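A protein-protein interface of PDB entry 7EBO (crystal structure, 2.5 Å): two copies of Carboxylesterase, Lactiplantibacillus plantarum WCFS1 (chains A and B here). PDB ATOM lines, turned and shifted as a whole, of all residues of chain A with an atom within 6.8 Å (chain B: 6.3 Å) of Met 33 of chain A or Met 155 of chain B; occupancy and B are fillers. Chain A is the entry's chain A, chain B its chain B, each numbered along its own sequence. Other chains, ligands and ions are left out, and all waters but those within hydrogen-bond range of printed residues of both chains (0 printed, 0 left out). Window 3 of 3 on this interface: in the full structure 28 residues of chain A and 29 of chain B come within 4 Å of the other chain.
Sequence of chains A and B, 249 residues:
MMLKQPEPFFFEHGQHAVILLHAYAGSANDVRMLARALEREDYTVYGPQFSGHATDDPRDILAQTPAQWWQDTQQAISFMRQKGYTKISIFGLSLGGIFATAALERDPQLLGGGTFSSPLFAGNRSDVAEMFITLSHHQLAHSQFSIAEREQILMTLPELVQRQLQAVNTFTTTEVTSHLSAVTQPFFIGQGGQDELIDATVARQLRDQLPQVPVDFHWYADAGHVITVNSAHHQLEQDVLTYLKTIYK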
ATOM      1  N   PHE A   9      -0.458   3.561   7.460  1.00  0.00           N
ATOM      2  CA  PHE A   9      -1.324   3.318   8.605  1.00  0.00           C
ATOM      3  C   PHE A   9      -2.154   4.556   8.914  1.00  0.00           C
ATOM      4  O   PHE A   9      -1.750   5.686   8.628  1.00  0.00           O
ATOM      5  CB  PHE A   9      -0.515   2.889   9.848  1.00  0.00           C
ATOM      6  CG  PHE A   9       0.422   3.946  10.371  1.00  0.00           C
ATOM      7  CD1 PHE A   9       1.750   3.951   9.986  1.00  0.00           C
ATOM      8  CD2 PHE A   9      -0.021   4.938  11.234  1.00  0.00           C
ATOM      9  CE1 PHE A   9       2.620   4.917  10.449  1.00  0.00           C
ATOM     10  CE2 PHE A   9       0.844   5.902  11.695  1.00  0.00           C
ATOM     11  CZ  PHE A   9       2.166   5.892  11.304  1.00  0.00           C
ATOM     12  N   ALA A  28       6.463   3.983   6.079  1.00  0.00           N
ATOM     13  CA  ALA A  28       5.671   4.343   7.251  1.00  0.00           C
ATOM     14  C   ALA A  28       6.120   3.598   8.499  1.00  0.00           C
ATOM     15  O   ALA A  28       5.788   4.017   9.613  1.00  0.00           O
ATOM     16  CB  ALA A  28       4.190   4.076   6.988  1.00  0.00           C
ATOM     17  N   ASN A  29       6.869   2.504   8.338  1.00  0.00           N
ATOM     18  CA  ASN A  29       7.446   1.818   9.484  1.00  0.00           C
ATOM     19  C   ASN A  29       8.504   2.665  10.183  1.00  0.00           C
ATOM     20  O   ASN A  29       8.869   2.359  11.322  1.00  0.00           O
ATOM     21  CB  ASN A  29       8.038   0.471   9.054  1.00  0.00           C
ATOM     22  CG  ASN A  29       6.971  -0.554   8.693  1.00  0.00           C
ATOM     23  OD1 ASN A  29       5.810  -0.427   9.086  1.00  0.00           O
ATOM     24  ND2 ASN A  29       7.363  -1.578   7.942  1.00  0.00           N
ATOM     25  N   ASP A  30       9.010   3.717   9.527  1.00  0.00           N
ATOM     26  CA  ASP A  30       9.981   4.599  10.170  1.00  0.00           C
ATOM     27  C   ASP A  30       9.400   5.280  11.400  1.00  0.00           C
ATOM     28  O   ASP A  30      10.135   5.593  12.344  1.00  0.00           O
ATOM     29  CB  ASP A  30      10.468   5.656   9.179  1.00  0.00           C
ATOM     30  CG  ASP A  30      11.178   5.056   7.990  1.00  0.00           C
ATOM     31  OD1 ASP A  30      11.399   3.828   7.993  1.00  0.00           O
ATOM     32  OD2 ASP A  30      11.519   5.810   7.056  1.00  0.00           O
ATOM     33  N   VAL A  31       8.086   5.495  11.418  1.00  0.00           N
ATOM     34  CA  VAL A  31       7.420   6.322  12.411  1.00  0.00           C
ATOM     35  C   VAL A  31       6.292   5.574  13.104  1.00  0.00           C
ATOM     36  O   VAL A  31       5.481   6.186  13.797  1.00  0.00           O
ATOM     37  CB  VAL A  31       6.900   7.632  11.786  1.00  0.00           C
ATOM     38  CG1 VAL A  31       8.059   8.510  11.338  1.00  0.00           C
ATOM     39  CG2 VAL A  31       5.979   7.326  10.618  1.00  0.00           C
ATOM     40  N   ARG A  32       6.215   4.256  12.915  1.00  0.00           N
ATOM     41  CA  ARG A  32       5.103   3.498  13.475  1.00  0.00           C
ATOM     42  C   ARG A  32       5.187   3.432  14.994  1.00  0.00           C
ATOM     43  O   ARG A  32       4.167   3.551  15.683  1.00  0.00           O
ATOM     44  CB  ARG A  32       5.076   2.094  12.880  1.00  0.00           C
ATOM     45  CG  ARG A  32       3.727   1.422  12.968  1.00  0.00           C
ATOM     46  CD  ARG A  32       3.686   0.231  12.042  1.00  0.00           C
ATOM     47  NE  ARG A  32       2.336  -0.283  11.869  1.00  0.00           N
ATOM     48  CZ  ARG A  32       1.743  -0.390  10.685  1.00  0.00           C
ATOM     49  NH1 ARG A  32       2.392  -0.020   9.590  1.00  0.00           N
ATOM     50  NH2 ARG A  32       0.510  -0.865  10.591  1.00  0.00           N
ATOM     51  N   MET A  33       6.390   3.213  15.532  1.00  0.00           N
ATOM     52  CA  MET A  33       6.557   3.157  16.981  1.00  0.00           C
ATOM     53  C   MET A  33       6.227   4.499  17.624  1.00  0.00           C
ATOM     54  O   MET A  33       5.587   4.549  18.681  1.00  0.00           O
ATOM     55  CB  MET A  33       7.977   2.717  17.323  1.00  0.00           C
ATOM     56  CG  MET A  33       8.249   2.577  18.809  1.00  0.00           C
ATOM     57  SD  MET A  33       9.868   1.853  19.112  1.00  0.00           S
ATOM     58  CE  MET A  33      10.810   2.682  17.840  1.00  0.00           C
ATOM     59  N   LEU A  34       6.679   5.599  17.011  1.00  0.00           N
ATOM     60  CA  LEU A  34       6.269   6.926  17.462  1.00  0.00           C
ATOM     61  C   LEU A  34       4.756   7.065  17.383  1.00  0.00           C
ATOM     62  O   LEU A  34       4.126   7.645  18.276  1.00  0.00           O
ATOM     63  CB  LEU A  34       6.955   8.003  16.617  1.00  0.00           C
ATOM     64  CG  LEU A  34       7.172   9.428  17.149  1.00  0.00           C
ATOM     65  CD1 LEU A  34       6.726  10.472  16.126  1.00  0.00           C
ATOM     66  CD2 LEU A  34       6.500   9.678  18.495  1.00  0.00           C
ATOM     67  N   ALA A  35       4.158   6.546  16.307  1.00  0.00           N
ATOM     68  CA  ALA A  35       2.709   6.592  16.155  1.00  0.00           C
ATOM     69  C   ALA A  35       2.006   5.885  17.307  1.00  0.00           C
ATOM     70  O   ALA A  35       0.977   6.358  17.802  1.00  0.00           O
ATOM     71  CB  ALA A  35       2.315   5.960  14.823  1.00  0.00           C
ATOM     72  N   ARG A  36       2.543   4.743  17.743  1.00  0.00           N
ATOM     73  CA  ARG A  36       1.946   4.029  18.867  1.00  0.00           C
ATOM     74  C   ARG A  36       2.038   4.831  20.157  1.00  0.00           C
ATOM     75  O   ARG A  36       1.107   4.811  20.969  1.00  0.00           O
ATOM     76  CB  ARG A  36       2.594   2.658  19.036  1.00  0.00           C
ATOM     77  CG  ARG A  36       2.062   1.617  18.084  1.00  0.00           C
ATOM     78  CD  ARG A  36       0.927   0.881  18.775  1.00  0.00           C
ATOM     79  NE  ARG A  36       1.419   0.165  19.947  1.00  0.00           N
ATOM     80  CZ  ARG A  36       1.835  -1.096  19.919  1.00  0.00           C
ATOM     81  NH1 ARG A  36       1.805  -1.773  18.781  1.00  0.00           N
ATOM     82  NH2 ARG A  36       2.280  -1.681  21.022  1.00  0.00           N
ATOM     83  N   ALA A  37       3.151   5.535  20.370  1.00  0.00           N
ATOM     84  CA  ALA A  37       3.266   6.340  21.580  1.00  0.00           C
ATOM     85  C   ALA A  37       2.244   7.468  21.595  1.00  0.00           C
ATOM     86  O   ALA A  37       1.727   7.822  22.661  1.00  0.00           O
ATOM     87  CB  ALA A  37       4.682   6.899  21.708  1.00  0.00           C
ATOM     88  N   LEU A  38       1.938   8.041  20.430  1.00  0.00           N
ATOM     89  CA  LEU A  38       0.888   9.050  20.355  1.00  0.00           C
ATOM     90  C   LEU A  38      -0.493   8.415  20.439  1.00  0.00           C
ATOM     91  O   LEU A  38      -1.418   9.004  21.012  1.00  0.00           O
ATOM     92  CB  LEU A  38       1.019   9.854  19.062  1.00  0.00           C
ATOM     93  CG  LEU A  38       2.380  10.484  18.766  1.00  0.00           C
ATOM     94  CD1 LEU A  38       2.316  11.312  17.490  1.00  0.00           C
ATOM     95  CD2 LEU A  38       2.874  11.315  19.939  1.00  0.00           C
ATOM     96  N   ILE A 227      16.225   8.895  15.058  1.00  0.00           N
ATOM     97  CA  ILE A 227      15.810   8.939  16.456  1.00  0.00           C
ATOM     98  C   ILE A 227      14.433   8.345  16.703  1.00  0.00           C
ATOM     99  O   ILE A 227      14.066   8.124  17.862  1.00  0.00           O
ATOM    100  CB  ILE A 227      15.864  10.398  16.953  1.00  0.00           C
ATOM    101  CG1 ILE A 227      15.241  11.338  15.917  1.00  0.00           C
ATOM    102  CG2 ILE A 227      17.289  10.798  17.275  1.00  0.00           C
ATOM    103  CD1 ILE A 227      15.173  12.784  16.370  1.00  0.00           C
ATOM    104  N   THR A 228      13.654   8.096  15.653  1.00  0.00           N
ATOM    105  CA  THR A 228      12.341   7.497  15.833  1.00  0.00           C
ATOM    106  C   THR A 228      12.418   6.004  16.108  1.00  0.00           C
ATOM    107  O   THR A 228      11.448   5.436  16.622  1.00  0.00           O
ATOM    108  CB  THR A 228      11.465   7.748  14.603  1.00  0.00           C
ATOM    109  OG1 THR A 228      12.115   7.235  13.435  1.00  0.00           O
ATOM    110  CG2 THR A 228      11.203   9.242  14.431  1.00  0.00           C
ATOM    111  N   VAL A 229      13.538   5.359  15.786  1.00  0.00           N
ATOM    112  CA  VAL A 229      13.664   3.916  15.974  1.00  0.00           C
ATOM    113  C   VAL A 229      14.858   3.514  16.826  1.00  0.00           C
ATOM    114  O   VAL A 229      14.902   2.368  17.303  1.00  0.00           O
ATOM    115  CB  VAL A 229      13.723   3.192  14.606  1.00  0.00           C
ATOM    116  CG1 VAL A 229      12.636   3.705  13.665  1.00  0.00           C
ATOM    117  CG2 VAL A 229      15.108   3.330  13.976  1.00  0.00           C
ATOM    118  N   ASN A 230      15.838   4.382  17.066  1.00  0.00           N
ATOM    119  CA  ASN A 230      17.046   3.998  17.784  1.00  0.00           C
ATOM    120  C   ASN A 230      16.843   4.174  19.293  1.00  0.00           C
ATOM    121  O   ASN A 230      15.710   4.222  19.779  1.00  0.00           O
ATOM    122  CB  ASN A 230      18.246   4.779  17.231  1.00  0.00           C
ATOM    123  CG  ASN A 230      18.166   6.279  17.498  1.00  0.00           C
ATOM    124  OD1 ASN A 230      17.441   6.741  18.379  1.00  0.00           O
ATOM    125  ND2 ASN A 230      18.926   7.046  16.727  1.00  0.00           N
ATOM    126  N   HIS A 233      14.350   6.831  20.927  1.00  0.00           N
ATOM    127  CA  HIS A 233      12.927   6.879  20.607  1.00  0.00           C
ATOM    128  C   HIS A 233      12.070   7.101  21.851  1.00  0.00           C
ATOM    129  O   HIS A 233      11.053   7.799  21.788  1.00  0.00           O
ATOM    130  CB  HIS A 233      12.511   5.611  19.855  1.00  0.00           C
ATOM    131  CG  HIS A 233      12.258   4.424  20.731  1.00  0.00           C
ATOM    132  ND1 HIS A 233      11.048   4.202  21.354  1.00  0.00           N
ATOM    133  CD2 HIS A 233      13.050   3.379  21.067  1.00  0.00           C
ATOM    134  CE1 HIS A 233      11.111   3.080  22.048  1.00  0.00           C
ATOM    135  NE2 HIS A 233      12.315   2.561  21.891  1.00  0.00           N
ATOM    136  N   HIS A 234      12.470   6.539  22.995  1.00  0.00           N
ATOM    137  CA  HIS A 234      11.707   6.760  24.222  1.00  0.00           C
ATOM    138  C   HIS A 234      11.694   8.232  24.621  1.00  0.00           C
ATOM    139  O   HIS A 234      10.636   8.790  24.935  1.00  0.00           O
ATOM    140  CB  HIS A 234      12.264   5.906  25.364  1.00  0.00           C
ATOM    141  CG  HIS A 234      11.797   4.484  25.347  1.00  0.00           C
ATOM    142  ND1 HIS A 234      12.634   3.419  25.090  1.00  0.00           N
ATOM    143  CD2 HIS A 234      10.575   3.951  25.583  1.00  0.00           C
ATOM    144  CE1 HIS A 234      11.945   2.294  25.159  1.00  0.00           C
ATOM    145  NE2 HIS A 234      10.693   2.589  25.455  1.00  0.00           N
ATOM    146  N   GLU A 237       9.703  10.323  22.013  1.00  0.00           N
ATOM    147  CA  GLU A 237       8.260  10.156  22.158  1.00  0.00           C
ATOM    148  C   GLU A 237       7.718  11.040  23.273  1.00  0.00           C
ATOM    149  O   GLU A 237       6.680  11.690  23.112  1.00  0.00           O
ATOM    150  CB  GLU A 237       7.936   8.687  22.424  1.00  0.00           C
ATOM    151  CG  GLU A 237       8.063   7.794  21.200  1.00  0.00           C
ATOM    152  CD  GLU A 237       8.403   6.364  21.563  1.00  0.00           C
ATOM    153  OE1 GLU A 237       8.133   5.968  22.715  1.00  0.00           O
ATOM    154  OE2 GLU A 237       8.953   5.640  20.705  1.00  0.00           O
ATOM    155  N   ARG B 150       3.448  -8.316  12.052  1.00  0.00           N
ATOM    156  CA  ARG B 150       4.545  -7.430  11.676  1.00  0.00           C
ATOM    157  C   ARG B 150       4.687  -6.289  12.673  1.00  0.00           C
ATOM    158  O   ARG B 150       5.805  -5.910  13.041  1.00  0.00           O
ATOM    159  CB  ARG B 150       4.318  -6.879  10.270  1.00  0.00           C
ATOM    160  CG  ARG B 150       4.337  -7.922   9.168  1.00  0.00           C
ATOM    161  CD  ARG B 150       3.819  -7.326   7.869  1.00  0.00           C
ATOM    162  NE  ARG B 150       3.975  -8.234   6.737  1.00  0.00           N
ATOM    163  CZ  ARG B 150       3.503  -7.992   5.518  1.00  0.00           C
ATOM    164  NH1 ARG B 150       3.686  -8.875   4.545  1.00  0.00           N
ATOM    165  NH2 ARG B 150       2.853  -6.864   5.269  1.00  0.00           N
ATOM    166  N   GLU B 151       3.560  -5.726  13.112  1.00  0.00           N
ATOM    167  CA  GLU B 151       3.597  -4.650  14.093  1.00  0.00           C
ATOM    168  C   GLU B 151       4.133  -5.138  15.435  1.00  0.00           C
ATOM    169  O   GLU B 151       4.913  -4.436  16.091  1.00  0.00           O
ATOM    170  CB  GLU B 151       2.195  -4.067  14.260  1.00  0.00           C
ATOM    171  CG  GLU B 151       2.123  -2.561  14.162  1.00  0.00           C
ATOM    172  CD  GLU B 151       1.337  -1.961  15.303  1.00  0.00           C
ATOM    173  OE1 GLU B 151       1.596  -2.348  16.462  1.00  0.00           O
ATOM    174  OE2 GLU B 151       0.455  -1.118  15.043  1.00  0.00           O
ATOM    175  N   GLN B 152       3.730  -6.341  15.859  1.00  0.00           N
ATOM    176  CA  GLN B 152       4.239  -6.896  17.112  1.00  0.00           C
ATOM    177  C   GLN B 152       5.749  -7.095  17.058  1.00  0.00           C
ATOM    178  O   GLN B 152       6.460  -6.792  18.023  1.00  0.00           O
ATOM    179  CB  GLN B 152       3.527  -8.212  17.437  1.00  0.00           C
ATOM    180  CG  GLN B 152       4.085  -8.960  18.649  1.00  0.00           C
ATOM    181  CD  GLN B 152       5.102 -10.024  18.283  1.00  0.00           C
ATOM    182  OE1 GLN B 152       4.961 -10.710  17.272  1.00  0.00           O
ATOM    183  NE2 GLN B 152       6.131 -10.171  19.110  1.00  0.00           N
ATOM    184  N   ILE B 153       6.256  -7.606  15.935  1.00  0.00           N
ATOM    185  CA  ILE B 153       7.693  -7.820  15.786  1.00  0.00           C
ATOM    186  C   ILE B 153       8.430  -6.486  15.755  1.00  0.00           C
ATOM    187  O   ILE B 153       9.446  -6.305  16.437  1.00  0.00           O
ATOM    188  CB  ILE B 153       7.980  -8.668  14.534  1.00  0.00           C
ATOM    189  CG1 ILE B 153       7.344 -10.052  14.676  1.00  0.00           C
ATOM    190  CG2 ILE B 153       9.474  -8.798  14.312  1.00  0.00           C
ATOM    191  CD1 ILE B 153       7.222 -10.809  13.372  1.00  0.00           C
ATOM    192  N   LEU B 154       7.946  -5.539  14.943  1.00  0.00           N
ATOM    193  CA  LEU B 154       8.662  -4.279  14.757  1.00  0.00           C
ATOM    194  C   LEU B 154       8.751  -3.500  16.065  1.00  0.00           C
ATOM    195  O   LEU B 154       9.732  -2.780  16.291  1.00  0.00           O
ATOM    196  CB  LEU B 154       7.999  -3.453  13.647  1.00  0.00           C
ATOM    197  CG  LEU B 154       7.464  -2.020  13.802  1.00  0.00           C
ATOM    198  CD1 LEU B 154       8.539  -0.967  14.059  1.00  0.00           C
ATOM    199  CD2 LEU B 154       6.692  -1.642  12.553  1.00  0.00           C
ATOM    200  N   MET B 155       7.758  -3.644  16.946  1.00  0.00           N
ATOM    201  CA  MET B 155       7.750  -2.895  18.198  1.00  0.00           C
ATOM    202  C   MET B 155       8.755  -3.427  19.209  1.00  0.00           C
ATOM    203  O   MET B 155       9.044  -2.731  20.189  1.00  0.00           O
ATOM    204  CB  MET B 155       6.358  -2.935  18.829  1.00  0.00           C
ATOM    205  CG  MET B 155       5.299  -2.112  18.124  1.00  0.00           C
ATOM    206  SD  MET B 155       5.693  -0.356  18.099  1.00  0.00           S
ATOM    207  CE  MET B 155       5.411   0.053  19.822  1.00  0.00           C
ATOM    208  N   THR B 156       9.294  -4.629  18.999  1.00  0.00           N
ATOM    209  CA  THR B 156      10.330  -5.174  19.864  1.00  0.00           C
ATOM    210  C   THR B 156      11.729  -4.988  19.299  1.00  0.00           C
ATOM    211  O   THR B 156      12.705  -5.200  20.026  1.00  0.00           O
ATOM    212  CB  THR B 156      10.106  -6.672  20.093  1.00  0.00           C
ATOM    213  OG1 THR B 156      10.399  -7.380  18.882  1.00  0.00           O
ATOM    214  CG2 THR B 156       8.669  -6.942  20.482  1.00  0.00           C
ATOM    215  N   LEU B 157      11.852  -4.589  18.034  1.00  0.00           N
ATOM    216  CA  LEU B 157      13.174  -4.532  17.416  1.00  0.00           C
ATOM    217  C   LEU B 157      14.098  -3.524  18.087  1.00  0.00           C
ATOM    218  O   LEU B 157      15.188  -3.929  18.523  1.00  0.00           O
ATOM    219  CB  LEU B 157      13.029  -4.246  15.916  1.00  0.00           C
ATOM    220  CG  LEU B 157      12.258  -5.268  15.073  1.00  0.00           C
ATOM    221  CD1 LEU B 157      12.266  -4.886  13.591  1.00  0.00           C
ATOM    222  CD2 LEU B 157      12.799  -6.682  15.282  1.00  0.00           C
ATOM    223  N   PRO B 158      13.718  -2.251  18.283  1.00  0.00           N
ATOM    224  CA  PRO B 158      14.704  -1.267  18.771  1.00  0.00           C
ATOM    225  C   PRO B 158      15.437  -1.664  20.043  1.00  0.00           C
ATOM    226  O   PRO B 158      16.655  -1.462  20.132  1.00  0.00           O
ATOM    227  CB  PRO B 158      13.846  -0.016  18.995  1.00  0.00           C
ATOM    228  CG  PRO B 158      12.750  -0.156  18.023  1.00  0.00           C
ATOM    229  CD  PRO B 158      12.422  -1.611  17.996  1.00  0.00           C
ATOM    230  N   GLU B 159      14.738  -2.227  21.032  1.00  0.00           N
ATOM    231  CA  GLU B 159      15.410  -2.607  22.271  1.00  0.00           C
ATOM    232  C   GLU B 159      16.291  -3.838  22.079  1.00  0.00           C
ATOM    233  O   GLU B 159      17.408  -3.894  22.607  1.00  0.00           O
ATOM    234  CB  GLU B 159      14.395  -2.841  23.389  1.00  0.00           C
ATOM    235  CG  GLU B 159      15.073  -3.061  24.731  1.00  0.00           C
ATOM    236  CD  GLU B 159      14.140  -3.553  25.811  1.00  0.00           C
ATOM    237  OE1 GLU B 159      12.942  -3.195  25.790  1.00  0.00           O
ATOM    238  OE2 GLU B 159      14.616  -4.300  26.689  1.00  0.00           O
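NE of Arg 32 of chain A lies within salt-bridge range of OE2 of Glu 151 of chain B.
The guanidinium group (NH1) of Arg 36 of chain A sits close to the side-chain carboxylate (OE1) of Glu 151 of chain B (2.4 Å).
Of the 19 printed residues of chain A, 5 touch a printed residue of chain B.
Hydrophobic or aromatic side chains of chain A within 4 Å of the printed part of chain B: Met 33.
Among the printed residues, Asp or Glu carboxylates within 4 Å of a Lys or Arg side-chain nitrogen of the other chain: Arg 32 of chain A with Glu 151 of chain B (3.8 Å) and Arg 36 of chain A with Glu 151 of chain B (2.4 Å).
CD2 of Leu 154 of chain B touches OD1 of Asn 29 of chain A, at 3.8 Å.
Arg 32 of chain A touches Leu 154 of chain B.
Met 155 of chain B touches Met 33 of chain A (SD to CA, 3.8 Å).
Pro 158 of chain B touches Met 33 of chain A.
Met 155 of chain B touches Arg 36 of chain A (CG to NH1, 3.6 Å).
Val 229 of chain A touches Pro 158 of chain B (O to CB, 3.1 Å).
No position is printed for both chains.
Of the 8 pairs that touch across the chains among the printed residues, none has its exchanged pair printed and touching as well.
The guanidinium group of Arg 32 of chain A sits at hydrogen-bond distance from the side-chain amide oxygen of Asn 29 of chain A.
SD of Met 33 of chain A sits close to ND1 of His 233 of chain A, 3.5 Å away.
Of the printed residues of chain B, Asn 29 of chain A touches Leu 154.
Val 31 of chain A touches none of the printed residues of chain B.
Met 33 of chain A touches two residues of chain B.
Of the printed residues of chain B, Val 229 of chain A touches Pro 158 (3.1 Å).
Met 155 of chain B touches just these residues of chain A: Met 33 (3.8 Å) and Arg 36 (3.6 Å).
The nearest residue of chain A that does not touch Met 155 of chain B is Arg 32 of chain A (4.8 Å).
The nearest printed residue of chain A that does not touch Glu 151 of chain B is Asn 29 of chain A (6.6 Å).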
